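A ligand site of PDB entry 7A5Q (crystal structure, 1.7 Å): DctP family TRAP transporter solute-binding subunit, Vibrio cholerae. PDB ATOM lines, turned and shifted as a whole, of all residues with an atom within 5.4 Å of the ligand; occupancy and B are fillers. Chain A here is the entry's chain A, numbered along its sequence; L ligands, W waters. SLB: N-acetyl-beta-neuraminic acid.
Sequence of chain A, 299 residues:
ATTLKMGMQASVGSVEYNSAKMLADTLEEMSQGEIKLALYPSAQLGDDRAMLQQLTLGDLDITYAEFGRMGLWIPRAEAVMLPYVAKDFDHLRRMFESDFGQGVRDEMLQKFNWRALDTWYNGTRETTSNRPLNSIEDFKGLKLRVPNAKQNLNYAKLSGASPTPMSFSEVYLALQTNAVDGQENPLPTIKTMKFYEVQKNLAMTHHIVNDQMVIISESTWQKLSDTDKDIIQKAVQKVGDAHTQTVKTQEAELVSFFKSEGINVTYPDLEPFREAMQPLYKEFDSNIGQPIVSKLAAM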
ATOM      1  N   GLN A   9       6.061   5.466 -28.196  1.00  0.00           N
ATOM      2  CA  GLN A   9       6.919   5.048 -29.294  1.00  0.00           C
ATOM      3  C   GLN A   9       8.020   4.123 -28.825  1.00  0.00           C
ATOM      4  O   GLN A   9       8.530   3.318 -29.608  1.00  0.00           O
ATOM      5  CB  GLN A   9       7.545   6.294 -29.912  1.00  0.00           C
ATOM      6  CG  GLN A   9       6.538   7.135 -30.757  1.00  0.00           C
ATOM      7  CD  GLN A   9       7.323   8.028 -31.737  1.00  0.00           C
ATOM      8  OE1 GLN A   9       7.554   7.595 -32.865  1.00  0.00           O
ATOM      9  NE2 GLN A   9       7.729   9.249 -31.311  1.00  0.00           N
ATOM     10  N   ALA A  10       8.444   4.289 -27.574  1.00  0.00           N
ATOM     11  CA  ALA A  10       9.545   3.482 -27.041  1.00  0.00           C
ATOM     12  C   ALA A  10       9.169   1.992 -27.036  1.00  0.00           C
ATOM     13  O   ALA A  10       8.010   1.618 -27.000  1.00  0.00           O
ATOM     14  CB  ALA A  10       9.882   3.958 -25.618  1.00  0.00           C
ATOM     15  N   GLU A  16      11.467   4.027 -20.903  1.00  0.00           N
ATOM     16  CA  GLU A  16      10.091   4.518 -20.964  1.00  0.00           C
ATOM     17  C   GLU A  16       9.103   3.400 -20.764  1.00  0.00           C
ATOM     18  O   GLU A  16       8.077   3.561 -20.090  1.00  0.00           O
ATOM     19  CB  GLU A  16       9.784   5.159 -22.337  1.00  0.00           C
ATOM     20  CG  GLU A  16      10.620   6.483 -22.595  1.00  0.00           C
ATOM     21  CD  GLU A  16      11.832   6.215 -23.488  1.00  0.00           C
ATOM     22  OE1 GLU A  16      12.492   5.150 -23.324  1.00  0.00           O
ATOM     23  OE2 GLU A  16      12.133   7.075 -24.353  1.00  0.00           O
ATOM     24  N   ASP A  48       4.352  10.107 -31.475  1.00  0.00           N
ATOM     25  CA  ASP A  48       3.772  10.855 -30.343  1.00  0.00           C
ATOM     26  C   ASP A  48       2.716  11.853 -30.799  1.00  0.00           C
ATOM     27  O   ASP A  48       1.725  12.089 -30.090  1.00  0.00           O
ATOM     28  CB  ASP A  48       4.899  11.527 -29.552  1.00  0.00           C
ATOM     29  CG  ASP A  48       5.824  12.411 -30.428  1.00  0.00           C
ATOM     30  OD1 ASP A  48       6.661  13.177 -29.891  1.00  0.00           O
ATOM     31  OD2 ASP A  48       5.801  12.245 -31.679  1.00  0.00           O
ATOM     32  N   TYR A  64       3.093   9.723 -23.570  1.00  0.00           N
ATOM     33  CA  TYR A  64       4.257  10.551 -23.269  1.00  0.00           C
ATOM     34  C   TYR A  64       4.412  11.681 -24.293  1.00  0.00           C
ATOM     35  O   TYR A  64       4.151  11.507 -25.492  1.00  0.00           O
ATOM     36  CB  TYR A  64       5.530   9.723 -23.299  1.00  0.00           C
ATOM     37  CG  TYR A  64       5.734   8.669 -22.204  1.00  0.00           C
ATOM     38  CD1 TYR A  64       5.738   8.994 -20.863  1.00  0.00           C
ATOM     39  CD2 TYR A  64       6.079   7.354 -22.576  1.00  0.00           C
ATOM     40  CE1 TYR A  64       6.006   8.011 -19.887  1.00  0.00           C
ATOM     41  CE2 TYR A  64       6.364   6.391 -21.647  1.00  0.00           C
ATOM     42  CZ  TYR A  64       6.323   6.731 -20.307  1.00  0.00           C
ATOM     43  OH  TYR A  64       6.574   5.739 -19.412  1.00  0.00           O
ATOM     44  N   ALA A  65       4.896  12.846 -23.821  1.00  0.00           N
ATOM     45  CA  ALA A  65       5.315  13.881 -24.763  1.00  0.00           C
ATOM     46  C   ALA A  65       6.235  14.851 -24.047  1.00  0.00           C
ATOM     47  O   ALA A  65       5.957  15.249 -22.909  1.00  0.00           O
ATOM     48  CB  ALA A  65       4.093  14.648 -25.310  1.00  0.00           C
ATOM     49  N   GLU A  66       7.218  15.384 -24.775  1.00  0.00           N
ATOM     50  CA  GLU A  66       8.018  16.477 -24.219  1.00  0.00           C
ATOM     51  C   GLU A  66       7.237  17.762 -24.134  1.00  0.00           C
ATOM     52  O   GLU A  66       6.392  18.064 -24.970  1.00  0.00           O
ATOM     53  CB  GLU A  66       9.279  16.705 -25.067  1.00  0.00           C
ATOM     54  CG  GLU A  66       9.967  15.402 -25.411  1.00  0.00           C
ATOM     55  CD  GLU A  66      10.942  15.542 -26.542  1.00  0.00           C
ATOM     56  OE1 GLU A  66      10.975  16.624 -27.168  1.00  0.00           O
ATOM     57  OE2 GLU A  66      11.503  14.492 -26.905  1.00  0.00           O
ATOM     58  N   ARG A  69       7.350  19.646 -27.281  1.00  0.00           N
ATOM     59  CA  ARG A  69       6.508  19.120 -28.395  1.00  0.00           C
ATOM     60  C   ARG A  69       5.147  19.804 -28.478  1.00  0.00           C
ATOM     61  O   ARG A  69       4.441  19.736 -29.511  1.00  0.00           O
ATOM     62  CB  ARG A  69       6.366  17.612 -28.179  1.00  0.00           C
ATOM     63  CG  ARG A  69       5.708  16.884 -29.367  1.00  0.00           C
ATOM     64  CD  ARG A  69       6.685  16.990 -30.579  1.00  0.00           C
ATOM     65  NE  ARG A  69       6.688  15.667 -31.291  1.00  0.00           N
ATOM     66  CZ  ARG A  69       7.192  15.533 -32.530  1.00  0.00           C
ATOM     67  NH1 ARG A  69       7.591  16.667 -33.201  1.00  0.00           N
ATOM     68  NH2 ARG A  69       7.215  14.297 -33.108  1.00  0.00           N
ATOM     69  N   MET A  81      12.377  23.766 -26.361  1.00  0.00           N
ATOM     70  CA  MET A  81      13.158  22.746 -27.061  1.00  0.00           C
ATOM     71  C   MET A  81      14.125  23.369 -28.073  1.00  0.00           C
ATOM     72  O   MET A  81      14.781  22.650 -28.804  1.00  0.00           O
ATOM     73  CB  MET A  81      12.250  21.749 -27.784  1.00  0.00           C
ATOM     74  CG  MET A  81      12.864  20.343 -27.993  1.00  0.00           C
ATOM     75  SD  MET A  81      12.077  19.263 -29.217  1.00  0.00           S
ATOM     76  CE  MET A  81      10.320  19.355 -28.717  1.00  0.00           C
ATOM     77  N   ARG A 125      20.032  14.788 -25.394  1.00  0.00           N
ATOM     78  CA  ARG A 125      20.367  14.219 -26.684  1.00  0.00           C
ATOM     79  C   ARG A 125      21.830  14.468 -27.055  1.00  0.00           C
ATOM     80  O   ARG A 125      22.391  15.508 -26.791  1.00  0.00           O
ATOM     81  CB  ARG A 125      19.527  14.840 -27.781  1.00  0.00           C
ATOM     82  CG  ARG A 125      18.003  14.608 -27.409  1.00  0.00           C
ATOM     83  CD  ARG A 125      17.075  15.148 -28.519  1.00  0.00           C
ATOM     84  NE  ARG A 125      16.909  14.216 -29.674  1.00  0.00           N
ATOM     85  CZ  ARG A 125      15.921  13.314 -29.823  1.00  0.00           C
ATOM     86  NH1 ARG A 125      15.072  13.004 -28.857  1.00  0.00           N
ATOM     87  NH2 ARG A 125      15.819  12.675 -30.996  1.00  0.00           N
ATOM     88  N   ARG A 145      19.998  11.953 -39.474  1.00  0.00           N
ATOM     89  CA  ARG A 145      18.560  11.746 -39.262  1.00  0.00           C
ATOM     90  C   ARG A 145      18.090  12.573 -38.069  1.00  0.00           C
ATOM     91  O   ARG A 145      18.778  12.687 -37.068  1.00  0.00           O
ATOM     92  CB  ARG A 145      18.262  10.255 -39.038  1.00  0.00           C
ATOM     93  CG  ARG A 145      16.808   9.977 -38.755  1.00  0.00           C
ATOM     94  CD  ARG A 145      16.639  10.098 -37.150  1.00  0.00           C
ATOM     95  NE  ARG A 145      15.207   9.904 -36.805  1.00  0.00           N
ATOM     96  CZ  ARG A 145      14.734   9.879 -35.554  1.00  0.00           C
ATOM     97  NH1 ARG A 145      13.428   9.688 -35.349  1.00  0.00           N
ATOM     98  NH2 ARG A 145      15.560  10.117 -34.571  1.00  0.00           N
ATOM     99  N   PRO A 147      14.131  13.374 -35.890  1.00  0.00           N
ATOM    100  CA  PRO A 147      12.687  13.087 -35.857  1.00  0.00           C
ATOM    101  C   PRO A 147      11.915  14.159 -36.579  1.00  0.00           C
ATOM    102  O   PRO A 147      12.436  15.196 -37.055  1.00  0.00           O
ATOM    103  CB  PRO A 147      12.326  13.072 -34.364  1.00  0.00           C
ATOM    104  CG  PRO A 147      13.393  13.892 -33.767  1.00  0.00           C
ATOM    105  CD  PRO A 147      14.663  13.802 -34.594  1.00  0.00           C
ATOM    106  N   ALA A 149      10.509  16.868 -36.120  1.00  0.00           N
ATOM    107  CA  ALA A 149      10.484  17.831 -35.023  1.00  0.00           C
ATOM    108  C   ALA A 149      11.350  18.980 -35.507  1.00  0.00           C
ATOM    109  O   ALA A 149      12.524  18.744 -35.815  1.00  0.00           O
ATOM    110  CB  ALA A 149      11.066  17.206 -33.755  1.00  0.00           C
ATOM    111  N   ASN A 152      14.876  19.813 -33.713  1.00  0.00           N
ATOM    112  CA  ASN A 152      15.936  18.856 -34.048  1.00  0.00           C
ATOM    113  C   ASN A 152      16.435  19.113 -35.452  1.00  0.00           C
ATOM    114  O   ASN A 152      17.643  19.092 -35.706  1.00  0.00           O
ATOM    115  CB  ASN A 152      15.449  17.418 -33.958  1.00  0.00           C
ATOM    116  CG  ASN A 152      14.862  17.083 -32.580  1.00  0.00           C
ATOM    117  OD1 ASN A 152      13.895  17.687 -32.159  1.00  0.00           O
ATOM    118  ND2 ASN A 152      15.487  16.138 -31.905  1.00  0.00           N
ATOM    119  N   MET A 166      12.858  11.371 -40.222  1.00  0.00           N
ATOM    120  CA  MET A 166      12.245  10.082 -40.488  1.00  0.00           C
ATOM    121  C   MET A 166      11.767   9.505 -39.160  1.00  0.00           C
ATOM    122  O   MET A 166      12.306   9.827 -38.093  1.00  0.00           O
ATOM    123  CB  MET A 166      13.217   9.173 -41.199  1.00  0.00           C
ATOM    124  CG  MET A 166      14.185   8.647 -40.373  1.00  0.00           C
ATOM    125  SD  MET A 166      15.154   7.257 -41.107  1.00  0.00           S
ATOM    126  CE  MET A 166      15.947   8.149 -42.364  1.00  0.00           C
ATOM    127  N   SER A 167      10.788   8.646 -39.242  1.00  0.00           N
ATOM    128  CA  SER A 167      10.235   8.072 -38.009  1.00  0.00           C
ATOM    129  C   SER A 167      11.264   7.236 -37.230  1.00  0.00           C
ATOM    130  O   SER A 167      12.183   6.611 -37.784  1.00  0.00           O
ATOM    131  CB  SER A 167       9.019   7.204 -38.338  1.00  0.00           C
ATOM    132  OG  SER A 167       9.428   5.942 -38.797  1.00  0.00           O
ATOM    133  N   PHE A 168      11.095   7.254 -35.919  1.00  0.00           N
ATOM    134  CA  PHE A 168      11.968   6.534 -34.992  1.00  0.00           C
ATOM    135  C   PHE A 168      12.129   5.059 -35.366  1.00  0.00           C
ATOM    136  O   PHE A 168      13.218   4.495 -35.220  1.00  0.00           O
ATOM    137  CB  PHE A 168      11.321   6.700 -33.604  1.00  0.00           C
ATOM    138  CG  PHE A 168      12.138   6.196 -32.435  1.00  0.00           C
ATOM    139  CD1 PHE A 168      13.454   6.601 -32.235  1.00  0.00           C
ATOM    140  CD2 PHE A 168      11.510   5.372 -31.494  1.00  0.00           C
ATOM    141  CE1 PHE A 168      14.191   6.159 -31.096  1.00  0.00           C
ATOM    142  CE2 PHE A 168      12.194   4.926 -30.345  1.00  0.00           C
ATOM    143  CZ  PHE A 168      13.537   5.288 -30.150  1.00  0.00           C
ATOM    144  N   GLU A 184      20.536  11.430 -33.574  1.00  0.00           N
ATOM    145  CA  GLU A 184      20.701  12.184 -32.343  1.00  0.00           C
ATOM    146  C   GLU A 184      19.600  11.744 -31.359  1.00  0.00           C
ATOM    147  O   GLU A 184      18.450  11.728 -31.765  1.00  0.00           O
ATOM    148  CB  GLU A 184      20.809  13.674 -32.677  1.00  0.00           C
ATOM    149  CG  GLU A 184      19.737  14.229 -33.576  1.00  0.00           C
ATOM    150  CD  GLU A 184      18.486  14.609 -32.792  1.00  0.00           C
ATOM    151  OE1 GLU A 184      17.410  14.383 -33.303  1.00  0.00           O
ATOM    152  OE2 GLU A 184      18.625  15.063 -31.665  1.00  0.00           O
ATOM    153  N   ASN A 185      20.036  11.346 -30.173  1.00  0.00           N
ATOM    154  CA  ASN A 185      19.114  10.831 -29.154  1.00  0.00           C
ATOM    155  C   ASN A 185      19.823  10.768 -27.788  1.00  0.00           C
ATOM    156  O   ASN A 185      21.026  10.811 -27.780  1.00  0.00           O
ATOM    157  CB  ASN A 185      18.589   9.438 -29.516  1.00  0.00           C
ATOM    158  CG  ASN A 185      17.214   9.419 -30.125  1.00  0.00           C
ATOM    159  OD1 ASN A 185      16.272   9.936 -29.543  1.00  0.00           O
ATOM    160  ND2 ASN A 185      17.085   8.823 -31.293  1.00  0.00           N
ATOM    161  N   PRO A 186      19.114  10.705 -26.623  1.00  0.00           N
ATOM    162  CA  PRO A 186      19.781  10.516 -25.362  1.00  0.00           C
ATOM    163  C   PRO A 186      20.481   9.144 -25.337  1.00  0.00           C
ATOM    164  O   PRO A 186      20.140   8.215 -26.079  1.00  0.00           O
ATOM    165  CB  PRO A 186      18.642  10.577 -24.333  1.00  0.00           C
ATOM    166  CG  PRO A 186      17.468  11.233 -25.106  1.00  0.00           C
ATOM    167  CD  PRO A 186      17.633  10.739 -26.498  1.00  0.00           C
ATOM    168  N   THR A 189      18.427   5.793 -24.953  1.00  0.00           N
ATOM    169  CA  THR A 189      17.760   5.439 -26.201  1.00  0.00           C
ATOM    170  C   THR A 189      18.757   4.824 -27.172  1.00  0.00           C
ATOM    171  O   THR A 189      18.466   3.807 -27.792  1.00  0.00           O
ATOM    172  CB  THR A 189      17.112   6.678 -26.791  1.00  0.00           C
ATOM    173  OG1 THR A 189      16.210   7.150 -25.801  1.00  0.00           O
ATOM    174  CG2 THR A 189      16.309   6.414 -28.189  1.00  0.00           C
ATOM    175  N   ASN A 210      15.684  16.498 -23.136  1.00  0.00           N
ATOM    176  CA  ASN A 210      14.307  15.997 -23.244  1.00  0.00           C
ATOM    177  C   ASN A 210      13.710  15.754 -21.845  1.00  0.00           C
ATOM    178  O   ASN A 210      14.234  14.994 -21.062  1.00  0.00           O
ATOM    179  CB  ASN A 210      14.254  14.684 -24.045  1.00  0.00           C
ATOM    180  CG  ASN A 210      14.527  14.806 -25.499  1.00  0.00           C
ATOM    181  OD1 ASN A 210      14.917  13.806 -26.086  1.00  0.00           O
ATOM    182  ND2 ASN A 210      14.261  15.969 -26.128  1.00  0.00           N
ATOM    183  N   GLN A 212       9.799  14.563 -20.288  1.00  0.00           N
ATOM    184  CA  GLN A 212       8.851  13.536 -20.709  1.00  0.00           C
ATOM    185  C   GLN A 212       7.603  13.765 -19.858  1.00  0.00           C
ATOM    186  O   GLN A 212       7.513  13.269 -18.729  1.00  0.00           O
ATOM    187  CB  GLN A 212       9.414  12.145 -20.504  1.00  0.00           C
ATOM    188  CG  GLN A 212       8.803  11.011 -21.309  1.00  0.00           C
ATOM    189  CD  GLN A 212       9.322  10.927 -22.756  1.00  0.00           C
ATOM    190  OE1 GLN A 212       9.984  11.840 -23.293  1.00  0.00           O
ATOM    191  NE2 GLN A 212       8.977   9.842 -23.381  1.00  0.00           N
HETATM  192  C1  SLB L   1      13.131  10.014 -31.869  1.00  0.00           C
HETATM  193  C2  SLB L   1      12.619  10.269 -30.332  1.00  0.00           C
HETATM  194  C3  SLB L   1      11.982   8.959 -29.961  1.00  0.00           C
HETATM  195  C4  SLB L   1      11.238   9.353 -28.702  1.00  0.00           C
HETATM  196  C5  SLB L   1      10.230  10.517 -29.065  1.00  0.00           C
HETATM  197  C6  SLB L   1      11.032  11.733 -29.441  1.00  0.00           C
HETATM  198  C7  SLB L   1      10.120  12.938 -29.751  1.00  0.00           C
HETATM  199  C8  SLB L   1      11.040  14.072 -30.256  1.00  0.00           C
HETATM  200  C9  SLB L   1      10.228  15.328 -30.503  1.00  0.00           C
HETATM  201  C10 SLB L   1       8.217  10.517 -27.629  1.00  0.00           C
HETATM  202  C11 SLB L   1       7.519  10.910 -26.330  1.00  0.00           C
HETATM  203  N5  SLB L   1       9.521  10.866 -27.790  1.00  0.00           N
HETATM  204  O1A SLB L   1      14.363  10.003 -32.035  1.00  0.00           O
HETATM  205  O1B SLB L   1      12.292   9.838 -32.808  1.00  0.00           O
HETATM  206  O2  SLB L   1      13.717  10.539 -29.609  1.00  0.00           O
HETATM  207  O4  SLB L   1      10.550   8.183 -28.179  1.00  0.00           O
HETATM  208  O6  SLB L   1      11.794  11.365 -30.637  1.00  0.00           O
HETATM  209  O7  SLB L   1       9.177  12.566 -30.763  1.00  0.00           O
HETATM  210  O8  SLB L   1      12.091  14.347 -29.288  1.00  0.00           O
HETATM  211  O9  SLB L   1       9.667  15.815 -29.244  1.00  0.00           O
HETATM  212  O10 SLB L   1       7.579   9.881 -28.485  1.00  0.00           O
HETATM  213  O   HOH W   1      10.021   8.435 -25.419  1.00  0.00           O
HETATM  214  O   HOH W   2      13.930  16.257 -29.326  1.00  0.00           O
HETATM  215  O   HOH W   3       9.792  10.882 -32.739  1.00  0.00           O
HETATM  216  O   HOH W   4      11.158  12.039 -25.808  1.00  0.00           O
HETATM  217  O   HOH W   5       5.891   8.204 -27.320  1.00  0.00           O
HETATM  218  O   HOH W   6      12.762   6.985 -26.872  1.00  0.00           O
HETATM  219  O   HOH W   7       7.684  14.350 -27.543  1.00  0.00           O
HETATM  220  O   HOH W   8      14.673   9.074 -27.041  1.00  0.00           O
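The side-chain carboxylate (OE2) of Glu 66 is in hydrogen-bond range of an oxygen (O8) of the ligand, 2.5 Å away.
OD1 of Asn 185 lies within hydrogen-bond range of O2 of the ligand.
OD1 of Asp 48 sits at hydrogen-bond distance from O7 of the ligand.
An oxygen (O1B) of the ligand lies within salt-bridge range of the guanidinium group (NH1) of Arg 145 (2.8 Å).
O10 of the ligand lies within hydrogen-bond range of NE2 of Gln 9 (2.9 Å).
An oxygen (O1A) of the ligand is in salt-bridge range of the guanidinium group (NH2) of Arg 125, 3.2 Å away.
ND2 of Asn 210 is in hydrogen-bond range of OE2 of Glu 66 (3.2 Å).
N of Asp 48 lies close to NE2 of Gln 9, 3.5 Å away.
The guanidinium group (NE) of Arg 69 lies within salt-bridge range of the side-chain carboxylate (OD1) of Asp 48, at 2.9 Å.
The backbone carbonyl oxygen (O) of Met 166 lies within hydrogen-bond range of the guanidinium group (NH1) of Arg 145.
The guanidinium group (NH1) of Arg 125 sits at hydrogen-bond distance from the side-chain amide oxygen (OD1) of Asn 210, at 2.9 Å.
The side-chain carboxylate of Glu 184 lies within salt-bridge range of the guanidinium group of Arg 125 (2.8 Å).
The side-chain amide nitrogen of Asn 152 sits close to the guanidinium group of Arg 125, at 3.3 Å.
The side-chain hydroxyl (OH) of Tyr 64 lies within hydrogen-bond range of the backbone carbonyl oxygen (O) of Glu 16, 2.7 Å away.
Merely in contact with the ligand: Phe 168 (3.4 Å), Gln 212 (3.5 Å), Arg 69 (3.5 Å), Tyr 64 (3.5 Å), Pro 147 (3.6 Å), Met 81 (3.6 Å) and Ala 149 (3.8 Å).
13 residues have an atom within 4 Å of the ligand: Gln 9, Asp 48, Tyr 64, Glu 66, Arg 69, Met 81, Arg 125, Arg 145, Pro 147, Ala 149, Phe 168, Asn 185 and Gln 212.
Water W3 lies within hydrogen-bond range of an oxygen (O7) of the ligand (2.7 Å) and the side-chain amide nitrogen of Gln 9 (3.0 Å).
Water W1 lies within hydrogen-bond range of NE2 of Gln 212, OE2 of Glu 16 and O4 of the ligand.
Water W4 lies within hydrogen-bond range of the side-chain carboxylate (OE2) of Glu 66, the side-chain amide oxygen (OE1) of Gln 212 and a nitrogen (N5) of the ligand.
Water W6 bridges the side-chain carboxylate of Glu 16 (2.6 Å) and an oxygen (O4) of the ligand (2.8 Å).
Water W7 lies within hydrogen-bond range of the side-chain carboxylate of Asp 48, the backbone NH of Glu 66 and an oxygen (O9) of the ligand.
Water W8 lies within hydrogen-bond range of the side-chain hydroxyl (OG1) of Thr 189 (2.8 Å), the side-chain amide oxygen (OD1) of Asn 185 (3.1 Å) and an oxygen (O2) of the ligand (3.1 Å).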
